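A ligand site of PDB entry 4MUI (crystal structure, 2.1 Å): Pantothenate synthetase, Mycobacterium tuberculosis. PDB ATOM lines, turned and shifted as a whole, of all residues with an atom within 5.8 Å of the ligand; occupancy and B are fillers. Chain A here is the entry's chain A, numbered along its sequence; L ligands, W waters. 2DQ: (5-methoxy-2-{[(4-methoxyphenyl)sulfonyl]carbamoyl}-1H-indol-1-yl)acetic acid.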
ATOM      1  N   PRO A  38       8.844 -13.056 -25.241  1.00  0.00           N
ATOM      2  CA  PRO A  38       8.509 -11.644 -25.270  1.00  0.00           C
ATOM      3  C   PRO A  38       9.458 -10.864 -24.387  1.00  0.00           C
ATOM      4  O   PRO A  38       9.758 -11.275 -23.261  1.00  0.00           O
ATOM      5  CB  PRO A  38       7.087 -11.594 -24.713  1.00  0.00           C
ATOM      6  CG  PRO A  38       6.672 -13.039 -24.412  1.00  0.00           C
ATOM      7  CD  PRO A  38       7.897 -13.837 -24.403  1.00  0.00           C
ATOM      8  N   THR A  39       9.990  -9.769 -24.919  1.00  0.00           N
ATOM      9  CA  THR A  39      10.821  -8.913 -24.096  1.00  0.00           C
ATOM     10  C   THR A  39      10.477  -7.418 -24.316  1.00  0.00           C
ATOM     11  O   THR A  39       9.901  -7.050 -25.345  1.00  0.00           O
ATOM     12  CB  THR A  39      12.343  -9.113 -24.395  1.00  0.00           C
ATOM     13  OG1 THR A  39      12.688  -8.438 -25.602  1.00  0.00           O
ATOM     14  CG2 THR A  39      12.752 -10.630 -24.489  1.00  0.00           C
ATOM     15  N   MET A  40      10.906  -6.596 -23.373  1.00  0.00           N
ATOM     16  CA  MET A  40      10.901  -5.170 -23.501  1.00  0.00           C
ATOM     17  C   MET A  40      12.286  -4.624 -23.788  1.00  0.00           C
ATOM     18  O   MET A  40      12.596  -3.534 -23.450  1.00  0.00           O
ATOM     19  CB  MET A  40      10.245  -4.499 -22.300  1.00  0.00           C
ATOM     20  CG  MET A  40       8.751  -4.678 -22.321  1.00  0.00           C
ATOM     21  SD  MET A  40       7.724  -3.599 -21.313  1.00  0.00           S
ATOM     22  CE  MET A  40       8.767  -3.533 -19.898  1.00  0.00           C
ATOM     23  N   GLY A  41      13.112  -5.395 -24.457  1.00  0.00           N
ATOM     24  CA  GLY A  41      14.416  -4.913 -24.906  1.00  0.00           C
ATOM     25  C   GLY A  41      15.389  -4.809 -23.732  1.00  0.00           C
ATOM     26  O   GLY A  41      15.118  -5.376 -22.639  1.00  0.00           O
ATOM     27  N   LEU A  43      18.423  -6.325 -23.234  1.00  0.00           N
ATOM     28  CA  LEU A  43      18.520  -7.754 -22.936  1.00  0.00           C
ATOM     29  C   LEU A  43      19.721  -8.104 -22.071  1.00  0.00           C
ATOM     30  O   LEU A  43      20.839  -7.589 -22.259  1.00  0.00           O
ATOM     31  CB  LEU A  43      18.582  -8.568 -24.222  1.00  0.00           C
ATOM     32  CG  LEU A  43      17.372  -8.616 -25.180  1.00  0.00           C
ATOM     33  CD1 LEU A  43      17.618  -9.624 -26.332  1.00  0.00           C
ATOM     34  CD2 LEU A  43      16.053  -8.950 -24.448  1.00  0.00           C
ATOM     35  N   HIS A  44      19.490  -8.965 -21.085  1.00  0.00           N
ATOM     36  CA  HIS A  44      20.565  -9.401 -20.254  1.00  0.00           C
ATOM     37  C   HIS A  44      20.628 -10.916 -20.306  1.00  0.00           C
ATOM     38  O   HIS A  44      19.988 -11.543 -21.168  1.00  0.00           O
ATOM     39  CB  HIS A  44      20.383  -8.877 -18.833  1.00  0.00           C
ATOM     40  CG  HIS A  44      19.013  -9.108 -18.280  1.00  0.00           C
ATOM     41  ND1 HIS A  44      18.100  -8.085 -18.108  1.00  0.00           N
ATOM     42  CD2 HIS A  44      18.404 -10.240 -17.842  1.00  0.00           C
ATOM     43  CE1 HIS A  44      16.988  -8.583 -17.590  1.00  0.00           C
ATOM     44  NE2 HIS A  44      17.144  -9.887 -17.428  1.00  0.00           N
ATOM     45  N   GLU A  45      21.377 -11.506 -19.385  1.00  0.00           N
ATOM     46  CA  GLU A  45      21.591 -12.946 -19.334  1.00  0.00           C
ATOM     47  C   GLU A  45      20.324 -13.764 -18.985  1.00  0.00           C
ATOM     48  O   GLU A  45      20.220 -14.950 -19.353  1.00  0.00           O
ATOM     49  CB  GLU A  45      22.725 -13.204 -18.329  1.00  0.00           C
ATOM     50  CG  GLU A  45      22.903 -14.641 -17.924  1.00  0.00           C
ATOM     51  CD  GLU A  45      23.559 -15.493 -19.001  1.00  0.00           C
ATOM     52  OE1 GLU A  45      24.026 -14.917 -20.009  1.00  0.00           O
ATOM     53  OE2 GLU A  45      23.592 -16.732 -18.830  1.00  0.00           O
ATOM     54  N   GLY A  46      19.372 -13.120 -18.275  1.00  0.00           N
ATOM     55  CA  GLY A  46      18.051 -13.735 -18.019  1.00  0.00           C
ATOM     56  C   GLY A  46      17.240 -14.018 -19.290  1.00  0.00           C
ATOM     57  O   GLY A  46      16.670 -15.073 -19.450  1.00  0.00           O
ATOM     58  N   HIS A  47      17.213 -13.040 -20.180  1.00  0.00           N
ATOM     59  CA  HIS A  47      16.640 -13.221 -21.508  1.00  0.00           C
ATOM     60  C   HIS A  47      17.351 -14.269 -22.307  1.00  0.00           C
ATOM     61  O   HIS A  47      16.687 -15.027 -23.011  1.00  0.00           O
ATOM     62  CB  HIS A  47      16.604 -11.901 -22.292  1.00  0.00           C
ATOM     63  CG  HIS A  47      15.871 -10.824 -21.568  1.00  0.00           C
ATOM     64  ND1 HIS A  47      16.472  -9.630 -21.208  1.00  0.00           N
ATOM     65  CD2 HIS A  47      14.601 -10.777 -21.097  1.00  0.00           C
ATOM     66  CE1 HIS A  47      15.586  -8.888 -20.577  1.00  0.00           C
ATOM     67  NE2 HIS A  47      14.448  -9.555 -20.483  1.00  0.00           N
ATOM     68  N   ALA A  49      18.768 -16.849 -21.126  1.00  0.00           N
ATOM     69  CA  ALA A  49      18.324 -18.129 -20.566  1.00  0.00           C
ATOM     70  C   ALA A  49      16.915 -18.476 -21.044  1.00  0.00           C
ATOM     71  O   ALA A  49      16.607 -19.629 -21.219  1.00  0.00           O
ATOM     72  CB  ALA A  49      18.336 -18.077 -19.030  1.00  0.00           C
ATOM     73  N   LEU A  50      16.050 -17.491 -21.214  1.00  0.00           N
ATOM     74  CA  LEU A  50      14.704 -17.696 -21.784  1.00  0.00           C
ATOM     75  C   LEU A  50      14.857 -18.227 -23.192  1.00  0.00           C
ATOM     76  O   LEU A  50      14.185 -19.181 -23.593  1.00  0.00           O
ATOM     77  CB  LEU A  50      13.935 -16.348 -21.893  1.00  0.00           C
ATOM     78  CG  LEU A  50      13.624 -15.547 -20.609  1.00  0.00           C
ATOM     79  CD1 LEU A  50      12.567 -14.490 -20.929  1.00  0.00           C
ATOM     80  CD2 LEU A  50      13.133 -16.451 -19.509  1.00  0.00           C
ATOM     81  N   GLN A  72       1.515  -0.342 -20.226  1.00  0.00           N
ATOM     82  CA  GLN A  72       1.741  -0.829 -18.853  1.00  0.00           C
ATOM     83  C   GLN A  72       2.419   0.234 -17.940  1.00  0.00           C
ATOM     84  O   GLN A  72       2.653  -0.028 -16.738  1.00  0.00           O
ATOM     85  CB  GLN A  72       2.506  -2.163 -18.871  1.00  0.00           C
ATOM     86  CG  GLN A  72       3.866  -2.117 -19.542  1.00  0.00           C
ATOM     87  CD  GLN A  72       4.476  -3.510 -19.773  1.00  0.00           C
ATOM     88  OE1 GLN A  72       5.413  -3.919 -19.070  1.00  0.00           O
ATOM     89  NE2 GLN A  72       3.937  -4.260 -20.753  1.00  0.00           N
ATOM     90  N   TYR A  82      12.642   4.251 -19.383  1.00  0.00           N
ATOM     91  CA  TYR A  82      12.940   2.846 -19.624  1.00  0.00           C
ATOM     92  C   TYR A  82      14.209   2.579 -20.467  1.00  0.00           C
ATOM     93  O   TYR A  82      14.430   3.286 -21.473  1.00  0.00           O
ATOM     94  CB  TYR A  82      11.715   2.133 -20.232  1.00  0.00           C
ATOM     95  CG  TYR A  82      11.739   0.675 -19.936  1.00  0.00           C
ATOM     96  CD1 TYR A  82      11.372   0.187 -18.662  1.00  0.00           C
ATOM     97  CD2 TYR A  82      12.219  -0.233 -20.873  1.00  0.00           C
ATOM     98  CE1 TYR A  82      11.451  -1.196 -18.357  1.00  0.00           C
ATOM     99  CE2 TYR A  82      12.290  -1.604 -20.586  1.00  0.00           C
ATOM    100  CZ  TYR A  82      11.896  -2.075 -19.334  1.00  0.00           C
ATOM    101  OH  TYR A  82      11.983  -3.422 -19.065  1.00  0.00           O
ATOM    102  N   VAL A 139      -0.239  -4.898 -19.468  1.00  0.00           N
ATOM    103  CA  VAL A 139       0.612  -6.077 -19.705  1.00  0.00           C
ATOM    104  C   VAL A 139      -0.182  -7.231 -20.364  1.00  0.00           C
ATOM    105  O   VAL A 139       0.304  -7.806 -21.346  1.00  0.00           O
ATOM    106  CB  VAL A 139       1.222  -6.635 -18.369  1.00  0.00           C
ATOM    107  CG1 VAL A 139       1.973  -7.951 -18.588  1.00  0.00           C
ATOM    108  CG2 VAL A 139       2.143  -5.608 -17.719  1.00  0.00           C
ATOM    109  N   VAL A 142      -1.035  -6.455 -24.166  1.00  0.00           N
ATOM    110  CA  VAL A 142       0.097  -6.616 -25.075  1.00  0.00           C
ATOM    111  C   VAL A 142       0.472  -8.086 -25.231  1.00  0.00           C
ATOM    112  O   VAL A 142       0.676  -8.563 -26.337  1.00  0.00           O
ATOM    113  CB  VAL A 142       1.289  -5.610 -24.712  1.00  0.00           C
ATOM    114  CG1 VAL A 142       2.043  -6.026 -23.390  1.00  0.00           C
ATOM    115  CG2 VAL A 142       2.278  -5.430 -25.868  1.00  0.00           C
ATOM    116  N   VAL A 143       0.442  -8.857 -24.139  1.00  0.00           N
ATOM    117  CA  VAL A 143       0.816 -10.265 -24.228  1.00  0.00           C
ATOM    118  C   VAL A 143      -0.221 -11.010 -25.062  1.00  0.00           C
ATOM    119  O   VAL A 143       0.158 -11.756 -25.956  1.00  0.00           O
ATOM    120  CB  VAL A 143       0.965 -10.886 -22.792  1.00  0.00           C
ATOM    121  CG1 VAL A 143       0.998 -12.463 -22.801  1.00  0.00           C
ATOM    122  CG2 VAL A 143       2.180 -10.281 -22.079  1.00  0.00           C
ATOM    123  N   PHE A 157       8.625 -16.998 -20.015  1.00  0.00           N
ATOM    124  CA  PHE A 157       8.795 -15.894 -19.094  1.00  0.00           C
ATOM    125  C   PHE A 157       9.729 -16.275 -17.952  1.00  0.00           C
ATOM    126  O   PHE A 157       9.728 -17.438 -17.498  1.00  0.00           O
ATOM    127  CB  PHE A 157       7.444 -15.508 -18.538  1.00  0.00           C
ATOM    128  CG  PHE A 157       6.517 -14.880 -19.562  1.00  0.00           C
ATOM    129  CD1 PHE A 157       6.601 -13.519 -19.855  1.00  0.00           C
ATOM    130  CD2 PHE A 157       5.517 -15.632 -20.161  1.00  0.00           C
ATOM    131  CE1 PHE A 157       5.739 -12.922 -20.772  1.00  0.00           C
ATOM    132  CE2 PHE A 157       4.641 -15.050 -21.053  1.00  0.00           C
ATOM    133  CZ  PHE A 157       4.730 -13.710 -21.369  1.00  0.00           C
ATOM    134  N   GLY A 158      10.519 -15.303 -17.452  1.00  0.00           N
ATOM    135  CA  GLY A 158      11.283 -15.508 -16.225  1.00  0.00           C
ATOM    136  C   GLY A 158      10.373 -15.484 -15.006  1.00  0.00           C
ATOM    137  O   GLY A 158       9.306 -14.868 -15.036  1.00  0.00           O
ATOM    138  N   GLU A 159      10.781 -16.173 -13.932  1.00  0.00           N
ATOM    139  CA  GLU A 159      10.012 -16.190 -12.671  1.00  0.00           C
ATOM    140  C   GLU A 159      10.203 -14.940 -11.805  1.00  0.00           C
ATOM    141  O   GLU A 159       9.466 -14.735 -10.838  1.00  0.00           O
ATOM    142  CB  GLU A 159      10.383 -17.407 -11.849  1.00  0.00           C
ATOM    143  CG  GLU A 159       9.773 -18.661 -12.352  1.00  0.00           C
ATOM    144  CD  GLU A 159      10.180 -19.876 -11.502  1.00  0.00           C
ATOM    145  OE1 GLU A 159      10.916 -19.723 -10.493  1.00  0.00           O
ATOM    146  OE2 GLU A 159       9.824 -20.981 -11.919  1.00  0.00           O
ATOM    147  N   LYS A 160      11.069 -14.044 -12.198  1.00  0.00           N
ATOM    148  CA  LYS A 160      11.315 -12.886 -11.419  1.00  0.00           C
ATOM    149  C   LYS A 160      10.081 -12.022 -11.204  1.00  0.00           C
ATOM    150  O   LYS A 160       9.697 -11.809 -10.100  1.00  0.00           O
ATOM    151  CB  LYS A 160      12.456 -12.042 -11.931  1.00  0.00           C
ATOM    152  CG  LYS A 160      12.865 -11.049 -10.880  1.00  0.00           C
ATOM    153  CD  LYS A 160      13.635  -9.892 -11.410  1.00  0.00           C
ATOM    154  CE  LYS A 160      13.425  -8.731 -10.522  1.00  0.00           C
ATOM    155  NZ  LYS A 160      12.362  -7.928 -11.109  1.00  0.00           N
ATOM    156  N   ASP A 161       9.407 -11.718 -12.285  1.00  0.00           N
ATOM    157  CA  ASP A 161       8.133 -10.992 -12.147  1.00  0.00           C
ATOM    158  C   ASP A 161       7.079 -12.043 -11.983  1.00  0.00           C
ATOM    159  O   ASP A 161       6.322 -12.349 -12.909  1.00  0.00           O
ATOM    160  CB  ASP A 161       7.867 -10.115 -13.356  1.00  0.00           C
ATOM    161  CG  ASP A 161       8.944  -9.053 -13.522  1.00  0.00           C
ATOM    162  OD1 ASP A 161       8.921  -8.074 -12.783  1.00  0.00           O
ATOM    163  OD2 ASP A 161       9.879  -9.248 -14.336  1.00  0.00           O
ATOM    164  N   GLN A 164       3.258 -11.217 -12.418  1.00  0.00           N
ATOM    165  CA  GLN A 164       3.012 -11.110 -13.872  1.00  0.00           C
ATOM    166  C   GLN A 164       2.820 -12.463 -14.569  1.00  0.00           C
ATOM    167  O   GLN A 164       1.886 -12.612 -15.380  1.00  0.00           O
ATOM    168  CB  GLN A 164       4.163 -10.347 -14.533  1.00  0.00           C
ATOM    169  CG  GLN A 164       4.089 -10.280 -16.057  1.00  0.00           C
ATOM    170  CD  GLN A 164       5.214  -9.452 -16.597  1.00  0.00           C
ATOM    171  OE1 GLN A 164       5.138  -8.211 -16.587  1.00  0.00           O
ATOM    172  NE2 GLN A 164       6.319 -10.118 -16.977  1.00  0.00           N
ATOM    173  N   ILE A 168      -0.468 -14.086 -16.431  1.00  0.00           N
ATOM    174  CA  ILE A 168      -0.417 -14.582 -17.807  1.00  0.00           C
ATOM    175  C   ILE A 168      -0.952 -16.013 -17.883  1.00  0.00           C
ATOM    176  O   ILE A 168      -1.635 -16.345 -18.869  1.00  0.00           O
ATOM    177  CB  ILE A 168       1.020 -14.450 -18.454  1.00  0.00           C
ATOM    178  CG1 ILE A 168       1.352 -12.944 -18.637  1.00  0.00           C
ATOM    179  CG2 ILE A 168       1.158 -15.274 -19.789  1.00  0.00           C
ATOM    180  CD1 ILE A 168       2.882 -12.572 -18.938  1.00  0.00           C
ATOM    181  N   VAL A 184      10.765 -19.598 -16.382  1.00  0.00           N
ATOM    182  CA  VAL A 184      12.191 -19.958 -16.311  1.00  0.00           C
ATOM    183  C   VAL A 184      12.779 -19.414 -15.018  1.00  0.00           C
ATOM    184  O   VAL A 184      12.618 -18.209 -14.751  1.00  0.00           O
ATOM    185  CB  VAL A 184      12.916 -19.442 -17.514  1.00  0.00           C
ATOM    186  CG1 VAL A 184      14.512 -19.781 -17.478  1.00  0.00           C
ATOM    187  CG2 VAL A 184      12.239 -19.999 -18.722  1.00  0.00           C
ATOM    188  N   PRO A 185      13.461 -20.296 -14.212  1.00  0.00           N
ATOM    189  CA  PRO A 185      14.042 -19.851 -12.935  1.00  0.00           C
ATOM    190  C   PRO A 185      14.893 -18.608 -13.175  1.00  0.00           C
ATOM    191  O   PRO A 185      15.605 -18.510 -14.192  1.00  0.00           O
ATOM    192  CB  PRO A 185      14.905 -21.036 -12.473  1.00  0.00           C
ATOM    193  CG  PRO A 185      14.344 -22.264 -13.215  1.00  0.00           C
ATOM    194  CD  PRO A 185      13.756 -21.711 -14.511  1.00  0.00           C
ATOM    195  N   THR A 186      14.748 -17.644 -12.275  1.00  0.00           N
ATOM    196  CA  THR A 186      15.405 -16.332 -12.324  1.00  0.00           C
ATOM    197  C   THR A 186      16.955 -16.496 -12.306  1.00  0.00           C
ATOM    198  O   THR A 186      17.526 -17.181 -11.418  1.00  0.00           O
ATOM    199  CB  THR A 186      14.908 -15.544 -11.067  1.00  0.00           C
ATOM    200  OG1 THR A 186      13.474 -15.441 -11.099  1.00  0.00           O
ATOM    201  CG2 THR A 186      15.521 -14.129 -10.959  1.00  0.00           C
ATOM    202  N   VAL A 187      17.622 -15.908 -13.305  1.00  0.00           N
ATOM    203  CA  VAL A 187      19.087 -15.885 -13.408  1.00  0.00           C
ATOM    204  C   VAL A 187      19.582 -14.825 -12.430  1.00  0.00           C
ATOM    205  O   VAL A 187      19.010 -13.760 -12.330  1.00  0.00           O
ATOM    206  CB  VAL A 187      19.576 -15.492 -14.842  1.00  0.00           C
ATOM    207  CG1 VAL A 187      21.135 -15.368 -14.893  1.00  0.00           C
ATOM    208  CG2 VAL A 187      19.092 -16.460 -15.868  1.00  0.00           C
ATOM    209  N   ALA A 194      18.951 -10.753  -8.143  1.00  0.00           N
ATOM    210  CA  ALA A 194      18.131 -11.120  -9.326  1.00  0.00           C
ATOM    211  C   ALA A 194      18.454 -10.156 -10.472  1.00  0.00           C
ATOM    212  O   ALA A 194      18.525  -8.955 -10.266  1.00  0.00           O
ATOM    213  CB  ALA A 194      16.644 -11.052  -8.998  1.00  0.00           C
ATOM    214  N   MET A 195      18.777 -10.731 -11.644  1.00  0.00           N
ATOM    215  CA  MET A 195      18.918  -9.999 -12.908  1.00  0.00           C
ATOM    216  C   MET A 195      17.744  -9.072 -13.094  1.00  0.00           C
ATOM    217  O   MET A 195      16.588  -9.463 -12.992  1.00  0.00           O
ATOM    218  CB  MET A 195      18.932 -10.940 -14.126  1.00  0.00           C
ATOM    219  CG  MET A 195      20.242 -11.694 -14.387  1.00  0.00           C
ATOM    220  SD  MET A 195      21.696 -10.628 -14.307  1.00  0.00           S
ATOM    221  CE  MET A 195      23.013 -11.861 -14.527  1.00  0.00           C
ATOM    222  N   SER A 196      18.055  -7.820 -13.383  1.00  0.00           N
ATOM    223  CA  SER A 196      17.037  -6.893 -13.766  1.00  0.00           C
ATOM    224  C   SER A 196      17.612  -5.744 -14.560  1.00  0.00           C
ATOM    225  O   SER A 196      18.766  -5.348 -14.368  1.00  0.00           O
ATOM    226  CB  SER A 196      16.346  -6.343 -12.527  1.00  0.00           C
ATOM    227  OG  SER A 196      15.612  -5.205 -12.866  1.00  0.00           O
ATOM    228  N   SER A 197      16.780  -5.173 -15.426  1.00  0.00           N
ATOM    229  CA  SER A 197      17.085  -3.952 -16.182  1.00  0.00           C
ATOM    230  C   SER A 197      17.316  -2.794 -15.224  1.00  0.00           C
ATOM    231  O   SER A 197      18.094  -1.879 -15.526  1.00  0.00           O
ATOM    232  CB  SER A 197      15.942  -3.604 -17.176  1.00  0.00           C
ATOM    233  OG  SER A 197      14.746  -3.190 -16.506  1.00  0.00           O
ATOM    234  N   ARG A 198      16.647  -2.856 -14.070  1.00  0.00           N
ATOM    235  CA  ARG A 198      16.733  -1.786 -13.071  1.00  0.00           C
ATOM    236  C   ARG A 198      17.986  -1.778 -12.200  1.00  0.00           C
ATOM    237  O   ARG A 198      18.218  -0.808 -11.465  1.00  0.00           O
ATOM    238  CB  ARG A 198      15.530  -1.850 -12.128  1.00  0.00           C
ATOM    239  CG  ARG A 198      14.261  -1.283 -12.716  1.00  0.00           C
ATOM    240  CD  ARG A 198      13.277  -1.027 -11.612  1.00  0.00           C
ATOM    241  NE  ARG A 198      12.114  -0.306 -12.102  1.00  0.00           N
ATOM    242  CZ  ARG A 198      10.908  -0.314 -11.541  1.00  0.00           C
ATOM    243  NH1 ARG A 198      10.670  -1.022 -10.442  1.00  0.00           N
ATOM    244  NH2 ARG A 198       9.932   0.390 -12.102  1.00  0.00           N
HETATM  245  O   2DQ L   1      14.656  -7.574 -16.484  1.00  0.00           O
HETATM  246  C   2DQ L   1      14.034  -7.722 -15.441  1.00  0.00           C
HETATM  247  OXT 2DQ L   1      13.687  -6.841 -14.677  1.00  0.00           O
HETATM  248  CA  2DQ L   1      13.705  -9.118 -15.011  1.00  0.00           C
HETATM  249  N   2DQ L   1      13.620 -10.132 -16.093  1.00  0.00           N
HETATM  250  CBA 2DQ L   1      14.227 -11.300 -15.852  1.00  0.00           C
HETATM  251  CAM 2DQ L   1      14.972 -11.704 -14.795  1.00  0.00           C
HETATM  252  CAL 2DQ L   1      15.523 -12.978 -14.730  1.00  0.00           C
HETATM  253  CAW 2DQ L   1      15.306 -13.836 -15.808  1.00  0.00           C
HETATM  254  OAS 2DQ L   1      15.875 -15.070 -15.733  1.00  0.00           O
HETATM  255  CAB 2DQ L   1      15.286 -15.995 -16.594  1.00  0.00           C
HETATM  256  CAN 2DQ L   1      14.537 -13.342 -16.923  1.00  0.00           C
HETATM  257  CAZ 2DQ L   1      14.009 -12.089 -16.908  1.00  0.00           C
HETATM  258  CAO 2DQ L   1      13.256 -11.367 -17.790  1.00  0.00           C
HETATM  259  CAY 2DQ L   1      13.035 -10.146 -17.289  1.00  0.00           C
HETATM  260  CAU 2DQ L   1      12.284  -9.142 -17.857  1.00  0.00           C
HETATM  261  OAD 2DQ L   1      11.524  -8.449 -17.189  1.00  0.00           O
HETATM  262  NAQ 2DQ L   1      12.410  -8.946 -19.170  1.00  0.00           N
HETATM  263  SBC 2DQ L   1      11.490  -7.779 -19.988  1.00  0.00           S
HETATM  264  OAE 2DQ L   1      12.123  -7.615 -21.320  1.00  0.00           O
HETATM  265  OAF 2DQ L   1      11.466  -6.381 -19.433  1.00  0.00           O
HETATM  266  CAX 2DQ L   1       9.842  -8.301 -20.090  1.00  0.00           C
HETATM  267  CAJ 2DQ L   1       9.538  -9.593 -20.506  1.00  0.00           C
HETATM  268  CAH 2DQ L   1       8.188 -10.008 -20.611  1.00  0.00           C
HETATM  269  CAV 2DQ L   1       7.160  -9.098 -20.294  1.00  0.00           C
HETATM  270  OAR 2DQ L   1       5.848  -9.503 -20.365  1.00  0.00           O
HETATM  271  CAA 2DQ L   1       4.893  -8.427 -20.619  1.00  0.00           C
HETATM  272  CAI 2DQ L   1       7.493  -7.808 -19.862  1.00  0.00           C
HETATM  273  CAK 2DQ L   1       8.822  -7.388 -19.763  1.00  0.00           C
HETATM  274  O   HOH W   1       8.712  -7.975 -16.428  1.00  0.00           O
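An oxygen (OAS) of the ligand is in hydrogen-bond range of the backbone NH (N) of Val 187 (3.1 Å).
An oxygen (OXT) of the ligand is in salt-bridge range of the side-chain amino group (NZ) of Lys 160, 3.96 Å away.
NE2 of His 47 is in hydrogen-bond range of NAQ of the ligand, at 2.5 Å.
The backbone NH (N) of Met 40 is in hydrogen-bond range of an oxygen (OAE) of the ligand (2.6 Å).
An oxygen (O) of the ligand lies within hydrogen-bond range of the backbone NH (N) of Ser 197 (3.4 Å).
An oxygen (OXT) of the ligand lies within hydrogen-bond range of the side-chain hydroxyl (OG) of Ser 196 (3.1 Å).
An oxygen (OAF) of the ligand lies within hydrogen-bond range of the side-chain hydroxyl (OH) of Tyr 82, 3.0 Å away.
The side-chain amide nitrogen of Gln 164 is in hydrogen-bond range of an oxygen (OAR) of the ligand (3.5 Å).
OG1 of Thr 39 is in hydrogen-bond range of N of Gly 41 (3.3 Å).
The backbone NH (N) of Met 195 lies within hydrogen-bond range of the backbone carbonyl oxygen (O) of Val 187 (3.1 Å).
OG of Ser 196 sits at hydrogen-bond distance from N of Arg 198 (2.8 Å).
OE1 of Gln 72 lies close to SD of Met 40, at 3.2 Å.
O of Phe 157 sits at hydrogen-bond distance from N of Val 184, 2.6 Å away.
The backbone NH (N) of Glu 159 is in hydrogen-bond range of the backbone carbonyl oxygen (O) of Val 184, at 2.9 Å.
The side-chain hydroxyl (OG1) of Thr 186 is in hydrogen-bond range of the backbone NH (N) of Lys 160 (3.0 Å).
ND1 of His 47 lies within hydrogen-bond range of N of His 44 (3.1 Å).
OAD of the ligand lies close to OD2 of Asp 161 (3.4 Å).
Merely in contact with the ligand: Pro 38 (3.2 Å), Thr 39 (3.3 Å), Gly 41 (3.97 Å), His 44 (2.8 Å), Gly 46 (3.3 Å), Leu 50 (3.7 Å), Val 139 (3.6 Å), Val 143 (3.6 Å), Phe 157 (3.4 Å), Gly 158 (3.97 Å), Val 184 (3.9 Å), Pro 185 (3.5 Å), Thr 186 (3.7 Å) and Met 195 (3.3 Å).
Hydrophobic or aromatic side chains within 4 Å of the ligand: Met 40, His 44, His 47, Leu 50, Val 139, Val 143, Phe 157, Val 184 and Val 187.
23 residues have an atom within 4 Å of the ligand: Pro 38, Thr 39, Met 40, Gly 41, His 44, Gly 46, His 47, Leu 50, Tyr 82, Val 139, Val 143, Phe 157, Gly 158, Lys 160, Asp 161, Gln 164, Val 184, Pro 185, Thr 186, Val 187, Met 195, Ser 196 and Ser 197.
Along chain A the residues within 4 Å of the ligand span positions 38 to 197.
Water W1 lies within hydrogen-bond range of OD2 of Asp 161 (2.7 Å), OAD of the ligand (3.0 Å) and NE2 of Gln 164 (3.3 Å).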
